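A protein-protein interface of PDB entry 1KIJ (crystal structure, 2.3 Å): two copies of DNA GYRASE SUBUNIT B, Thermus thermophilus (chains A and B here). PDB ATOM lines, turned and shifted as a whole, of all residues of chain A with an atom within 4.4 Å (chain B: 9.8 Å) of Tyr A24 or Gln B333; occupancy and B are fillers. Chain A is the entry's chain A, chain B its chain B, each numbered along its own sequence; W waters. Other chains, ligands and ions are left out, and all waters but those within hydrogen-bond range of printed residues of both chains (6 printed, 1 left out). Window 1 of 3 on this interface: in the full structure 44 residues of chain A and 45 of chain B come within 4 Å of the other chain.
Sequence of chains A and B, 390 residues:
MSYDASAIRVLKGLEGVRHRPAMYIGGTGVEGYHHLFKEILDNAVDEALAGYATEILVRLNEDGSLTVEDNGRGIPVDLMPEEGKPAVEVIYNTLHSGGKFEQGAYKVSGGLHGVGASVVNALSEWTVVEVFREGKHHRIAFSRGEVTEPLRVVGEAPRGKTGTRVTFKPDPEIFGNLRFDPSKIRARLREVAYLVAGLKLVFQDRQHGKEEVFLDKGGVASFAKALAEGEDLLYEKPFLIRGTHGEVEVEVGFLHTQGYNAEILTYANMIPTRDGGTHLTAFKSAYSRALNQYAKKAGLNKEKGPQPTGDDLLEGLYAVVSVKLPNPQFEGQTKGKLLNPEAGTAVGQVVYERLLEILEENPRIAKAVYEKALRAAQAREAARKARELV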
ATOM      1  N   GLY A  16      -9.786   7.470  -5.782  1.00  0.00           N
ATOM      2  CA  GLY A  16      -9.692   6.118  -5.262  1.00  0.00           C
ATOM      3  C   GLY A  16      -9.932   5.038  -6.301  1.00  0.00           C
ATOM      4  O   GLY A  16      -9.346   3.973  -6.223  1.00  0.00           O
ATOM      5  N   VAL A  17     -10.807   5.306  -7.269  1.00  0.00           N
ATOM      6  CA  VAL A  17     -11.091   4.326  -8.316  1.00  0.00           C
ATOM      7  C   VAL A  17      -9.862   4.071  -9.197  1.00  0.00           C
ATOM      8  O   VAL A  17      -9.525   2.929  -9.485  1.00  0.00           O
ATOM      9  CB  VAL A  17     -12.265   4.782  -9.211  1.00  0.00           C
ATOM     10  CG1 VAL A  17     -12.437   3.803 -10.362  1.00  0.00           C
ATOM     11  CG2 VAL A  17     -13.555   4.868  -8.377  1.00  0.00           C
ATOM     12  N   ARG A  20      -7.106   2.242  -7.177  1.00  0.00           N
ATOM     13  CA  ARG A  20      -7.295   0.808  -6.980  1.00  0.00           C
ATOM     14  C   ARG A  20      -8.515   0.307  -7.745  1.00  0.00           C
ATOM     15  O   ARG A  20      -9.552   0.052  -7.172  1.00  0.00           O
ATOM     16  CB  ARG A  20      -7.437   0.505  -5.480  1.00  0.00           C
ATOM     17  CG  ARG A  20      -7.268  -0.972  -5.129  1.00  0.00           C
ATOM     18  CD  ARG A  20      -6.385  -1.160  -3.890  1.00  0.00           C
ATOM     19  NE  ARG A  20      -7.027  -0.728  -2.642  1.00  0.00           N
ATOM     20  CZ  ARG A  20      -7.936  -1.434  -1.969  1.00  0.00           C
ATOM     21  NH1 ARG A  20      -8.332  -2.623  -2.409  1.00  0.00           N
ATOM     22  NH2 ARG A  20      -8.448  -0.951  -0.846  1.00  0.00           N
ATOM     23  N   PRO A  21      -8.383   0.157  -9.069  1.00  0.00           N
ATOM     24  CA  PRO A  21      -9.487  -0.313  -9.910  1.00  0.00           C
ATOM     25  C   PRO A  21     -10.082  -1.674  -9.547  1.00  0.00           C
ATOM     26  O   PRO A  21     -11.300  -1.840  -9.576  1.00  0.00           O
ATOM     27  CB  PRO A  21      -8.881  -0.305 -11.309  1.00  0.00           C
ATOM     28  CG  PRO A  21      -7.857   0.811 -11.221  1.00  0.00           C
ATOM     29  CD  PRO A  21      -7.220   0.543  -9.893  1.00  0.00           C
ATOM     30  N   ALA A  22      -9.233  -2.642  -9.200  1.00  0.00           N
ATOM     31  CA  ALA A  22      -9.723  -3.982  -8.865  1.00  0.00           C
ATOM     32  C   ALA A  22     -10.734  -4.009  -7.715  1.00  0.00           C
ATOM     33  O   ALA A  22     -11.563  -4.911  -7.630  1.00  0.00           O
ATOM     34  CB  ALA A  22      -8.549  -4.912  -8.557  1.00  0.00           C
ATOM     35  N   MET A  23     -10.665  -3.030  -6.826  1.00  0.00           N
ATOM     36  CA  MET A  23     -11.609  -2.971  -5.719  1.00  0.00           C
ATOM     37  C   MET A  23     -13.006  -2.566  -6.214  1.00  0.00           C
ATOM     38  O   MET A  23     -13.997  -2.773  -5.527  1.00  0.00           O
ATOM     39  CB  MET A  23     -11.113  -1.973  -4.671  1.00  0.00           C
ATOM     40  CG  MET A  23     -12.012  -1.822  -3.448  1.00  0.00           C
ATOM     41  SD  MET A  23     -11.397  -0.528  -2.354  1.00  0.00           S
ATOM     42  CE  MET A  23     -12.049   0.916  -3.111  1.00  0.00           C
ATOM     43  N   TYR A  24     -13.075  -1.984  -7.408  1.00  0.00           N
ATOM     44  CA  TYR A  24     -14.348  -1.560  -7.986  1.00  0.00           C
ATOM     45  C   TYR A  24     -14.848  -2.490  -9.083  1.00  0.00           C
ATOM     46  O   TYR A  24     -16.046  -2.671  -9.237  1.00  0.00           O
ATOM     47  CB  TYR A  24     -14.237  -0.147  -8.571  1.00  0.00           C
ATOM     48  CG  TYR A  24     -14.188   0.958  -7.543  1.00  0.00           C
ATOM     49  CD1 TYR A  24     -12.982   1.369  -6.981  1.00  0.00           C
ATOM     50  CD2 TYR A  24     -15.362   1.579  -7.116  1.00  0.00           C
ATOM     51  CE1 TYR A  24     -12.951   2.378  -6.015  1.00  0.00           C
ATOM     52  CE2 TYR A  24     -15.342   2.579  -6.160  1.00  0.00           C
ATOM     53  CZ  TYR A  24     -14.139   2.971  -5.616  1.00  0.00           C
ATOM     54  OH  TYR A  24     -14.141   3.942  -4.663  1.00  0.00           O
ATOM     55  N   ILE A  25     -13.931  -3.065  -9.855  1.00  0.00           N
ATOM     56  CA  ILE A  25     -14.334  -3.951 -10.939  1.00  0.00           C
ATOM     57  C   ILE A  25     -13.764  -5.371 -10.857  1.00  0.00           C
ATOM     58  O   ILE A  25     -13.923  -6.155 -11.784  1.00  0.00           O
ATOM     59  CB  ILE A  25     -13.986  -3.329 -12.318  1.00  0.00           C
ATOM     60  CG1 ILE A  25     -12.492  -3.020 -12.398  1.00  0.00           C
ATOM     61  CG2 ILE A  25     -14.798  -2.038 -12.534  1.00  0.00           C
ATOM     62  CD1 ILE A  25     -12.061  -2.557 -13.754  1.00  0.00           C
ATOM     63  N   GLY A  26     -13.107  -5.687  -9.744  1.00  0.00           N
ATOM     64  CA  GLY A  26     -12.562  -7.020  -9.541  1.00  0.00           C
ATOM     65  C   GLY A  26     -11.171  -7.283 -10.081  1.00  0.00           C
ATOM     66  O   GLY A  26     -10.431  -8.085  -9.532  1.00  0.00           O
ATOM     67  N   LEU A  95     -18.209  10.173  -7.203  1.00  0.00           N
ATOM     68  CA  LEU A  95     -18.183   8.773  -6.828  1.00  0.00           C
ATOM     69  C   LEU A  95     -19.558   8.239  -6.440  1.00  0.00           C
ATOM     70  O   LEU A  95     -19.963   7.179  -6.905  1.00  0.00           O
ATOM     71  CB  LEU A  95     -17.198   8.572  -5.667  1.00  0.00           C
ATOM     72  CG  LEU A  95     -16.998   7.156  -5.118  1.00  0.00           C
ATOM     73  CD1 LEU A  95     -16.693   6.173  -6.244  1.00  0.00           C
ATOM     74  CD2 LEU A  95     -15.864   7.184  -4.117  1.00  0.00           C
ATOM     75  N   LEU A 112     -21.759  -1.063 -10.503  1.00  0.00           N
ATOM     76  CA  LEU A 112     -20.537  -0.501  -9.974  1.00  0.00           C
ATOM     77  C   LEU A 112     -20.952   0.554  -8.944  1.00  0.00           C
ATOM     78  O   LEU A 112     -22.094   1.048  -8.967  1.00  0.00           O
ATOM     79  CB  LEU A 112     -19.707   0.114 -11.106  1.00  0.00           C
ATOM     80  CG  LEU A 112     -19.219  -0.897 -12.158  1.00  0.00           C
ATOM     81  CD1 LEU A 112     -18.336  -0.207 -13.192  1.00  0.00           C
ATOM     82  CD2 LEU A 112     -18.451  -2.020 -11.470  1.00  0.00           C
ATOM     83  N   HIS A 113     -20.033   0.885  -8.043  1.00  0.00           N
ATOM     84  CA  HIS A 113     -20.273   1.858  -6.982  1.00  0.00           C
ATOM     85  C   HIS A 113     -21.272   2.950  -7.364  1.00  0.00           C
ATOM     86  O   HIS A 113     -21.117   3.612  -8.374  1.00  0.00           O
ATOM     87  CB  HIS A 113     -18.955   2.512  -6.576  1.00  0.00           C
ATOM     88  CG  HIS A 113     -18.950   3.040  -5.175  1.00  0.00           C
ATOM     89  ND1 HIS A 113     -18.734   2.233  -4.078  1.00  0.00           N
ATOM     90  CD2 HIS A 113     -19.139   4.289  -4.690  1.00  0.00           C
ATOM     91  CE1 HIS A 113     -18.786   2.962  -2.979  1.00  0.00           C
ATOM     92  NE2 HIS A 113     -19.031   4.214  -3.322  1.00  0.00           N
ATOM     93  N   VAL A 119     -17.670   5.565 -12.214  1.00  0.00           N
ATOM     94  CA  VAL A 119     -16.554   4.627 -12.137  1.00  0.00           C
ATOM     95  C   VAL A 119     -16.073   4.340 -13.573  1.00  0.00           C
ATOM     96  O   VAL A 119     -14.903   4.270 -13.827  1.00  0.00           O
ATOM     97  CB  VAL A 119     -16.973   3.290 -11.442  1.00  0.00           C
ATOM     98  CG1 VAL A 119     -15.910   2.214 -11.661  1.00  0.00           C
ATOM     99  CG2 VAL A 119     -17.155   3.514  -9.947  1.00  0.00           C
ATOM    100  N   THR A 334     -19.512 -10.719  -3.808  1.00  0.00           N
ATOM    101  CA  THR A 334     -20.102 -10.982  -5.152  1.00  0.00           C
ATOM    102  C   THR A 334     -21.526 -11.505  -5.358  1.00  0.00           C
ATOM    103  O   THR A 334     -21.762 -12.358  -6.203  1.00  0.00           O
ATOM    104  CB  THR A 334     -19.125 -11.734  -6.097  1.00  0.00           C
ATOM    105  OG1 THR A 334     -17.774 -11.464  -5.700  1.00  0.00           O
ATOM    106  CG2 THR A 334     -19.311 -11.284  -7.540  1.00  0.00           C
ATOM    107  N   GLY B  13     -17.795  10.875   1.319  1.00  0.00           N
ATOM    108  CA  GLY B  13     -17.216  10.021   2.342  1.00  0.00           C
ATOM    109  C   GLY B  13     -18.154   8.971   2.909  1.00  0.00           C
ATOM    110  O   GLY B  13     -18.923   8.352   2.182  1.00  0.00           O
ATOM    111  N   ALA B  22     -26.341  -1.691   2.070  1.00  0.00           N
ATOM    112  CA  ALA B  22     -26.303  -2.888   1.231  1.00  0.00           C
ATOM    113  C   ALA B  22     -25.246  -2.819   0.122  1.00  0.00           C
ATOM    114  O   ALA B  22     -24.743  -3.833  -0.323  1.00  0.00           O
ATOM    115  CB  ALA B  22     -27.677  -3.138   0.623  1.00  0.00           C
ATOM    116  N   MET B  23     -24.921  -1.612  -0.325  1.00  0.00           N
ATOM    117  CA  MET B  23     -23.916  -1.433  -1.365  1.00  0.00           C
ATOM    118  C   MET B  23     -22.497  -1.769  -0.874  1.00  0.00           C
ATOM    119  O   MET B  23     -21.600  -1.987  -1.670  1.00  0.00           O
ATOM    120  CB  MET B  23     -23.963   0.003  -1.871  1.00  0.00           C
ATOM    121  CG  MET B  23     -23.039   0.280  -3.036  1.00  0.00           C
ATOM    122  SD  MET B  23     -23.278   1.943  -3.657  1.00  0.00           S
ATOM    123  CE  MET B  23     -22.051   2.829  -2.780  1.00  0.00           C
ATOM    124  N   TYR B  24     -22.307  -1.805   0.442  1.00  0.00           N
ATOM    125  CA  TYR B  24     -20.999  -2.117   1.027  1.00  0.00           C
ATOM    126  C   TYR B  24     -20.924  -3.478   1.685  1.00  0.00           C
ATOM    127  O   TYR B  24     -19.865  -4.066   1.753  1.00  0.00           O
ATOM    128  CB  TYR B  24     -20.606  -1.067   2.065  1.00  0.00           C
ATOM    129  CG  TYR B  24     -20.291   0.283   1.472  1.00  0.00           C
ATOM    130  CD1 TYR B  24     -21.299   1.203   1.221  1.00  0.00           C
ATOM    131  CD2 TYR B  24     -18.985   0.625   1.138  1.00  0.00           C
ATOM    132  CE1 TYR B  24     -21.021   2.432   0.652  1.00  0.00           C
ATOM    133  CE2 TYR B  24     -18.694   1.849   0.572  1.00  0.00           C
ATOM    134  CZ  TYR B  24     -19.720   2.745   0.335  1.00  0.00           C
ATOM    135  OH  TYR B  24     -19.443   3.960  -0.213  1.00  0.00           O
ATOM    136  N   LEU B  95     -13.428   7.263   4.027  1.00  0.00           N
ATOM    137  CA  LEU B  95     -13.937   6.150   3.233  1.00  0.00           C
ATOM    138  C   LEU B  95     -12.802   5.340   2.602  1.00  0.00           C
ATOM    139  O   LEU B  95     -12.789   4.126   2.673  1.00  0.00           O
ATOM    140  CB  LEU B  95     -14.835   6.691   2.114  1.00  0.00           C
ATOM    141  CG  LEU B  95     -16.004   5.866   1.562  1.00  0.00           C
ATOM    142  CD1 LEU B  95     -16.096   6.106   0.057  1.00  0.00           C
ATOM    143  CD2 LEU B  95     -15.831   4.392   1.853  1.00  0.00           C
ATOM    144  N   HIS B  96     -11.843   6.033   1.999  1.00  0.00           N
ATOM    145  CA  HIS B  96     -10.755   5.354   1.315  1.00  0.00           C
ATOM    146  C   HIS B  96      -9.378   5.969   1.532  1.00  0.00           C
ATOM    147  O   HIS B  96      -9.088   7.064   1.071  1.00  0.00           O
ATOM    148  CB  HIS B  96     -11.063   5.300  -0.192  1.00  0.00           C
ATOM    149  CG  HIS B  96     -10.126   4.436  -0.980  1.00  0.00           C
ATOM    150  ND1 HIS B  96     -10.160   4.366  -2.356  1.00  0.00           N
ATOM    151  CD2 HIS B  96      -9.132   3.604  -0.587  1.00  0.00           C
ATOM    152  CE1 HIS B  96      -9.230   3.527  -2.777  1.00  0.00           C
ATOM    153  NE2 HIS B  96      -8.592   3.051  -1.723  1.00  0.00           N
ATOM    154  N   SER B  97      -8.533   5.249   2.257  1.00  0.00           N
ATOM    155  CA  SER B  97      -7.176   5.702   2.492  1.00  0.00           C
ATOM    156  C   SER B  97      -6.253   4.573   2.029  1.00  0.00           C
ATOM    157  O   SER B  97      -6.621   3.397   2.081  1.00  0.00           O
ATOM    158  CB  SER B  97      -6.955   6.053   3.974  1.00  0.00           C
ATOM    159  OG  SER B  97      -7.234   4.967   4.836  1.00  0.00           O
ATOM    160  N   SER B 109      -7.888 -10.680   1.267  1.00  0.00           N
ATOM    161  CA  SER B 109      -8.572 -10.072   0.129  1.00  0.00           C
ATOM    162  C   SER B 109     -10.053  -9.831   0.381  1.00  0.00           C
ATOM    163  O   SER B 109     -10.581 -10.217   1.410  1.00  0.00           O
ATOM    164  CB  SER B 109      -8.402 -10.940  -1.118  1.00  0.00           C
ATOM    165  OG  SER B 109      -7.166 -10.655  -1.738  1.00  0.00           O
ATOM    166  N   GLY B 110     -10.711  -9.191  -0.584  1.00  0.00           N
ATOM    167  CA  GLY B 110     -12.124  -8.900  -0.443  1.00  0.00           C
ATOM    168  C   GLY B 110     -12.343  -7.939   0.713  1.00  0.00           C
ATOM    169  O   GLY B 110     -11.578  -6.981   0.907  1.00  0.00           O
ATOM    170  N   GLY B 111     -13.383  -8.186   1.496  1.00  0.00           N
ATOM    171  CA  GLY B 111     -13.634  -7.305   2.616  1.00  0.00           C
ATOM    172  C   GLY B 111     -14.295  -6.008   2.196  1.00  0.00           C
ATOM    173  O   GLY B 111     -14.652  -5.817   1.043  1.00  0.00           O
ATOM    174  N   LEU B 112     -14.424  -5.100   3.149  1.00  0.00           N
ATOM    175  CA  LEU B 112     -15.080  -3.825   2.927  1.00  0.00           C
ATOM    176  C   LEU B 112     -14.219  -2.748   2.261  1.00  0.00           C
ATOM    177  O   LEU B 112     -13.007  -2.775   2.329  1.00  0.00           O
ATOM    178  CB  LEU B 112     -15.637  -3.327   4.269  1.00  0.00           C
ATOM    179  CG  LEU B 112     -16.964  -3.912   4.796  1.00  0.00           C
ATOM    180  CD1 LEU B 112     -17.206  -5.338   4.331  1.00  0.00           C
ATOM    181  CD2 LEU B 112     -16.956  -3.830   6.307  1.00  0.00           C
ATOM    182  N   HIS B 113     -14.893  -1.802   1.618  1.00  0.00           N
ATOM    183  CA  HIS B 113     -14.273  -0.679   0.915  1.00  0.00           C
ATOM    184  C   HIS B 113     -12.986  -0.141   1.570  1.00  0.00           C
ATOM    185  O   HIS B 113     -12.947   0.069   2.760  1.00  0.00           O
ATOM    186  CB  HIS B 113     -15.292   0.456   0.811  1.00  0.00           C
ATOM    187  CG  HIS B 113     -15.029   1.409  -0.312  1.00  0.00           C
ATOM    188  ND1 HIS B 113     -15.510   1.207  -1.585  1.00  0.00           N
ATOM    189  CD2 HIS B 113     -14.346   2.578  -0.349  1.00  0.00           C
ATOM    190  CE1 HIS B 113     -15.143   2.213  -2.358  1.00  0.00           C
ATOM    191  NE2 HIS B 113     -14.437   3.058  -1.633  1.00  0.00           N
ATOM    192  N   GLY B 114     -11.950   0.096   0.762  1.00  0.00           N
ATOM    193  CA  GLY B 114     -10.687   0.616   1.277  1.00  0.00           C
ATOM    194  C   GLY B 114     -10.083  -0.266   2.358  1.00  0.00           C
ATOM    195  O   GLY B 114      -9.913  -1.468   2.152  1.00  0.00           O
ATOM    196  N   ILE B 271      -9.680 -15.653   1.666  1.00  0.00           N
ATOM    197  CA  ILE B 271     -11.106 -15.596   1.389  1.00  0.00           C
ATOM    198  C   ILE B 271     -11.525 -16.792   0.550  1.00  0.00           C
ATOM    199  O   ILE B 271     -10.855 -17.159  -0.406  1.00  0.00           O
ATOM    200  CB  ILE B 271     -11.526 -14.274   0.660  1.00  0.00           C
ATOM    201  CG1 ILE B 271     -10.981 -14.249  -0.765  1.00  0.00           C
ATOM    202  CG2 ILE B 271     -11.017 -13.061   1.433  1.00  0.00           C
ATOM    203  CD1 ILE B 271     -11.267 -12.956  -1.496  1.00  0.00           C
ATOM    204  N   PRO B 272     -12.650 -17.429   0.914  1.00  0.00           N
ATOM    205  CA  PRO B 272     -13.132 -18.590   0.166  1.00  0.00           C
ATOM    206  C   PRO B 272     -13.394 -18.232  -1.297  1.00  0.00           C
ATOM    207  O   PRO B 272     -13.903 -17.164  -1.595  1.00  0.00           O
ATOM    208  CB  PRO B 272     -14.424 -18.961   0.894  1.00  0.00           C
ATOM    209  CG  PRO B 272     -14.211 -18.433   2.283  1.00  0.00           C
ATOM    210  CD  PRO B 272     -13.561 -17.107   2.025  1.00  0.00           C
ATOM    211  N   PRO B 328      -4.383  -9.756  -6.375  1.00  0.00           N
ATOM    212  CA  PRO B 328      -5.282 -10.806  -6.859  1.00  0.00           C
ATOM    213  C   PRO B 328      -6.356 -10.228  -7.801  1.00  0.00           C
ATOM    214  O   PRO B 328      -6.793  -9.100  -7.648  1.00  0.00           O
ATOM    215  CB  PRO B 328      -5.867 -11.371  -5.569  1.00  0.00           C
ATOM    216  CG  PRO B 328      -5.953 -10.158  -4.698  1.00  0.00           C
ATOM    217  CD  PRO B 328      -4.619  -9.474  -4.946  1.00  0.00           C
ATOM    218  N   GLN B 329      -6.749 -11.028  -8.780  1.00  0.00           N
ATOM    219  CA  GLN B 329      -7.747 -10.670  -9.782  1.00  0.00           C
ATOM    220  C   GLN B 329      -8.922 -11.627  -9.625  1.00  0.00           C
ATOM    221  O   GLN B 329      -8.751 -12.845  -9.669  1.00  0.00           O
ATOM    222  CB  GLN B 329      -7.156 -10.827 -11.188  1.00  0.00           C
ATOM    223  CG  GLN B 329      -5.849 -10.078 -11.404  1.00  0.00           C
ATOM    224  CD  GLN B 329      -6.056  -8.590 -11.611  1.00  0.00           C
ATOM    225  OE1 GLN B 329      -6.528  -8.161 -12.655  1.00  0.00           O
ATOM    226  NE2 GLN B 329      -5.708  -7.797 -10.605  1.00  0.00           N
ATOM    227  N   PHE B 330     -10.113 -11.076  -9.443  1.00  0.00           N
ATOM    228  CA  PHE B 330     -11.295 -11.901  -9.274  1.00  0.00           C
ATOM    229  C   PHE B 330     -12.316 -11.667 -10.377  1.00  0.00           C
ATOM    230  O   PHE B 330     -12.286 -10.642 -11.046  1.00  0.00           O
ATOM    231  CB  PHE B 330     -11.911 -11.625  -7.907  1.00  0.00           C
ATOM    232  CG  PHE B 330     -11.074 -12.119  -6.764  1.00  0.00           C
ATOM    233  CD1 PHE B 330     -10.958 -13.482  -6.512  1.00  0.00           C
ATOM    234  CD2 PHE B 330     -10.386 -11.225  -5.951  1.00  0.00           C
ATOM    235  CE1 PHE B 330     -10.169 -13.950  -5.463  1.00  0.00           C
ATOM    236  CE2 PHE B 330      -9.594 -11.685  -4.901  1.00  0.00           C
ATOM    237  CZ  PHE B 330      -9.486 -13.052  -4.657  1.00  0.00           C
ATOM    238  N   GLU B 331     -13.212 -12.636 -10.556  1.00  0.00           N
ATOM    239  CA  GLU B 331     -14.263 -12.568 -11.573  1.00  0.00           C
ATOM    240  C   GLU B 331     -15.017 -11.238 -11.549  1.00  0.00           C
ATOM    241  O   GLU B 331     -15.492 -10.772 -12.580  1.00  0.00           O
ATOM    242  CB  GLU B 331     -15.260 -13.729 -11.391  1.00  0.00           C
ATOM    243  CG  GLU B 331     -16.162 -13.643 -10.150  1.00  0.00           C
ATOM    244  CD  GLU B 331     -17.070 -14.867  -9.972  1.00  0.00           C
ATOM    245  OE1 GLU B 331     -17.763 -15.259 -10.941  1.00  0.00           O
ATOM    246  OE2 GLU B 331     -17.101 -15.436  -8.854  1.00  0.00           O
ATOM    247  N   GLY B 332     -15.118 -10.634 -10.367  1.00  0.00           N
ATOM    248  CA  GLY B 332     -15.813  -9.372 -10.224  1.00  0.00           C
ATOM    249  C   GLY B 332     -16.168  -9.133  -8.769  1.00  0.00           C
ATOM    250  O   GLY B 332     -16.591 -10.041  -8.074  1.00  0.00           O
ATOM    251  N   GLN B 333     -15.990  -7.900  -8.312  1.00  0.00           N
ATOM    252  CA  GLN B 333     -16.284  -7.545  -6.926  1.00  0.00           C
ATOM    253  C   GLN B 333     -15.424  -8.340  -5.936  1.00  0.00           C
ATOM    254  O   GLN B 333     -15.929  -8.914  -4.972  1.00  0.00           O
ATOM    255  CB  GLN B 333     -17.772  -7.754  -6.633  1.00  0.00           C
ATOM    256  CG  GLN B 333     -18.692  -7.030  -7.608  1.00  0.00           C
ATOM    257  CD  GLN B 333     -18.268  -5.589  -7.870  1.00  0.00           C
ATOM    258  OE1 GLN B 333     -18.188  -4.773  -6.953  1.00  0.00           O
ATOM    259  NE2 GLN B 333     -17.996  -5.275  -9.133  1.00  0.00           N
ATOM    260  N   THR B 334     -14.121  -8.361  -6.209  1.00  0.00           N
ATOM    261  CA  THR B 334     -13.100  -9.029  -5.396  1.00  0.00           C
ATOM    262  C   THR B 334     -13.494 -10.298  -4.622  1.00  0.00           C
ATOM    263  O   THR B 334     -13.373 -10.342  -3.403  1.00  0.00           O
ATOM    264  CB  THR B 334     -12.475  -8.017  -4.402  1.00  0.00           C
ATOM    265  OG1 THR B 334     -12.186  -6.791  -5.091  1.00  0.00           O
ATOM    266  CG2 THR B 334     -11.176  -8.564  -3.819  1.00  0.00           C
ATOM    267  N   LYS B 335     -13.943 -11.325  -5.344  1.00  0.00           N
ATOM    268  CA  LYS B 335     -14.337 -12.612  -4.759  1.00  0.00           C
ATOM    269  C   LYS B 335     -14.975 -13.520  -5.807  1.00  0.00           C
ATOM    270  O   LYS B 335     -15.339 -13.071  -6.897  1.00  0.00           O
ATOM    271  CB  LYS B 335     -15.328 -12.411  -3.604  1.00  0.00           C
ATOM    272  CG  LYS B 335     -14.682 -12.368  -2.222  1.00  0.00           C
ATOM    273  CD  LYS B 335     -15.637 -11.823  -1.162  1.00  0.00           C
ATOM    274  CE  LYS B 335     -14.966 -11.772   0.205  1.00  0.00           C
ATOM    275  NZ  LYS B 335     -15.799 -11.079   1.224  1.00  0.00           N
ATOM    276  N   GLY B 336     -15.100 -14.805  -5.474  1.00  0.00           N
ATOM    277  CA  GLY B 336     -15.719 -15.750  -6.390  1.00  0.00           C
ATOM    278  C   GLY B 336     -14.784 -16.725  -7.077  1.00  0.00           C
ATOM    279  O   GLY B 336     -14.646 -17.865  -6.650  1.00  0.00           O
ATOM    280  N   LYS B 337     -14.151 -16.271  -8.153  1.00  0.00           N
ATOM    281  CA  LYS B 337     -13.233 -17.098  -8.925  1.00  0.00           C
ATOM    282  C   LYS B 337     -11.896 -16.398  -9.182  1.00  0.00           C
ATOM    283  O   LYS B 337     -11.850 -15.311  -9.756  1.00  0.00           O
ATOM    284  CB  LYS B 337     -13.880 -17.479 -10.260  1.00  0.00           C
ATOM    285  CG  LYS B 337     -12.920 -18.080 -11.273  1.00  0.00           C
ATOM    286  CD  LYS B 337     -13.604 -18.343 -12.606  1.00  0.00           C
ATOM    287  CE  LYS B 337     -14.535 -19.542 -12.536  1.00  0.00           C
ATOM    288  NZ  LYS B 337     -13.784 -20.820 -12.349  1.00  0.00           N
ATOM    289  N   LEU B 339      -8.630 -15.482 -10.970  1.00  0.00           N
ATOM    290  CA  LEU B 339      -8.220 -15.475 -12.380  1.00  0.00           C
ATOM    291  C   LEU B 339      -6.712 -15.379 -12.658  1.00  0.00           C
ATOM    292  O   LEU B 339      -6.296 -15.596 -13.782  1.00  0.00           O
ATOM    293  CB  LEU B 339      -8.932 -14.345 -13.126  1.00  0.00           C
ATOM    294  CG  LEU B 339     -10.464 -14.311 -13.019  1.00  0.00           C
ATOM    295  CD1 LEU B 339     -10.978 -12.991 -13.577  1.00  0.00           C
ATOM    296  CD2 LEU B 339     -11.082 -15.491 -13.758  1.00  0.00           C
HETATM  297  O   HOH W   1      -9.222  -8.448  -6.647  1.00  0.00           O
HETATM  298  O   HOH W   2     -12.910   5.080  -2.864  1.00  0.00           O
HETATM  299  O   HOH W   3     -12.628  -8.778 -12.920  1.00  0.00           O
HETATM  300  O   HOH W   4     -24.317   0.616  -6.993  1.00  0.00           O
HETATM  301  O   HOH W   5      -6.452   1.311  -0.517  1.00  0.00           O
HETATM  302  O   HOH W   6     -14.147  -5.406  -6.783  1.00  0.00           O
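O of Gln B329 is in hydrogen-bond range of N of Leu B339, at 2.9 Å.
NH2 of Arg A20 sits at hydrogen-bond distance from SD of Met A23 (3.3 Å).
Ala A22 touches just one residue of chain B: Thr B334 (3.2 Å).
Of chain B, only His B113 (3.1 Å) and Gln B333 (3.3 Å) come within 4 Å of Tyr A24.
Ile A25 touches none of the printed residues of chain B.
Gly B13 touches none of the printed residues of chain A.
Of the printed residues of chain A, Gln B329 touches Gly A26.
The nearest residue of chain B that does not touch Tyr A24 is His B96 (4.6 Å).
The nearest residue of chain A that does not touch Gln B333 is Leu A112 (4.03 Å).
The nearest printed residue of chain A that does not touch His B96 is Arg A20 (4.1 Å).
O of Lys B335 sits at hydrogen-bond distance from OG1 of Thr A334 (3.2 Å).
The backbone carbonyl oxygen (O) of Tyr A24 sits at hydrogen-bond distance from the side-chain amide nitrogen (NE2) of Gln B333, at 3.3 Å.
O of Gly B332 lies within hydrogen-bond range of OG1 of Thr A334 (3.0 Å).
NE2 of His B113 lies close to OH of Tyr A24 (3.2 Å).
NH2 of Arg A20 sits at hydrogen-bond distance from O of Gly B114, at 3.4 Å.
O of Gln B333 sits at hydrogen-bond distance from OG1 of Thr A334, 3.2 Å away.
The side-chain sulfur (SD) of Met A23 lies within hydrogen-bond range of the backbone NH (N) of Gly B114, at 3.2 Å.
OG1 of Thr B334 lies within hydrogen-bond range of O of Ala A22, at 3.2 Å.
O of Gly A26 is in hydrogen-bond range of N of Phe B330, at 3.0 Å.
The side-chain hydroxyl (OH) of Tyr B24 sits close to a ring nitrogen (NE2) of His A113, 3.1 Å away.
Among the printed residues, merely in contact across the chains: Gly A16 with His B96, Met A23 with His B96, Met A23 with His B113, Met A23 with Thr B334, Gly A26 with Gln B329, Gly A26 with Gln B333, Gly A26 with Thr B334, His A113 with Met B23 and His A113 with His B113.
Of the 26 printed residues of chain B, 11 touch a printed residue of chain A.
Hydrophobic or aromatic side chains of chain B that line the printed part of chain A: Met B23, Tyr B24, His B96 and His B113.
Of the 14 printed residues of chain A, 8 touch a printed residue of chain B.
Along chain A the printed residues that touch a printed residue of chain B span positions 16 to 334.
Among the printed residues, 19 pairs touch across the chains.
Among the printed residues, no Asp or Glu carboxylate lies within 4 Å of a Lys or Arg side-chain nitrogen of the other chain.
Water W1 bridges O of Pro B328 (2.7 Å) and O of Gly A26 (3.1 Å).
Water W4 lies within hydrogen-bond range of the backbone carbonyl oxygen of Leu A112 (3.0 Å) and the side-chain sulfur of Met B23 (3.7 Å).
His B113 touches its own counterpart, His A113.
Of the 19 pairs that touch across the chains among the printed residues, 5 have their exchanged pair printed and touching as well.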
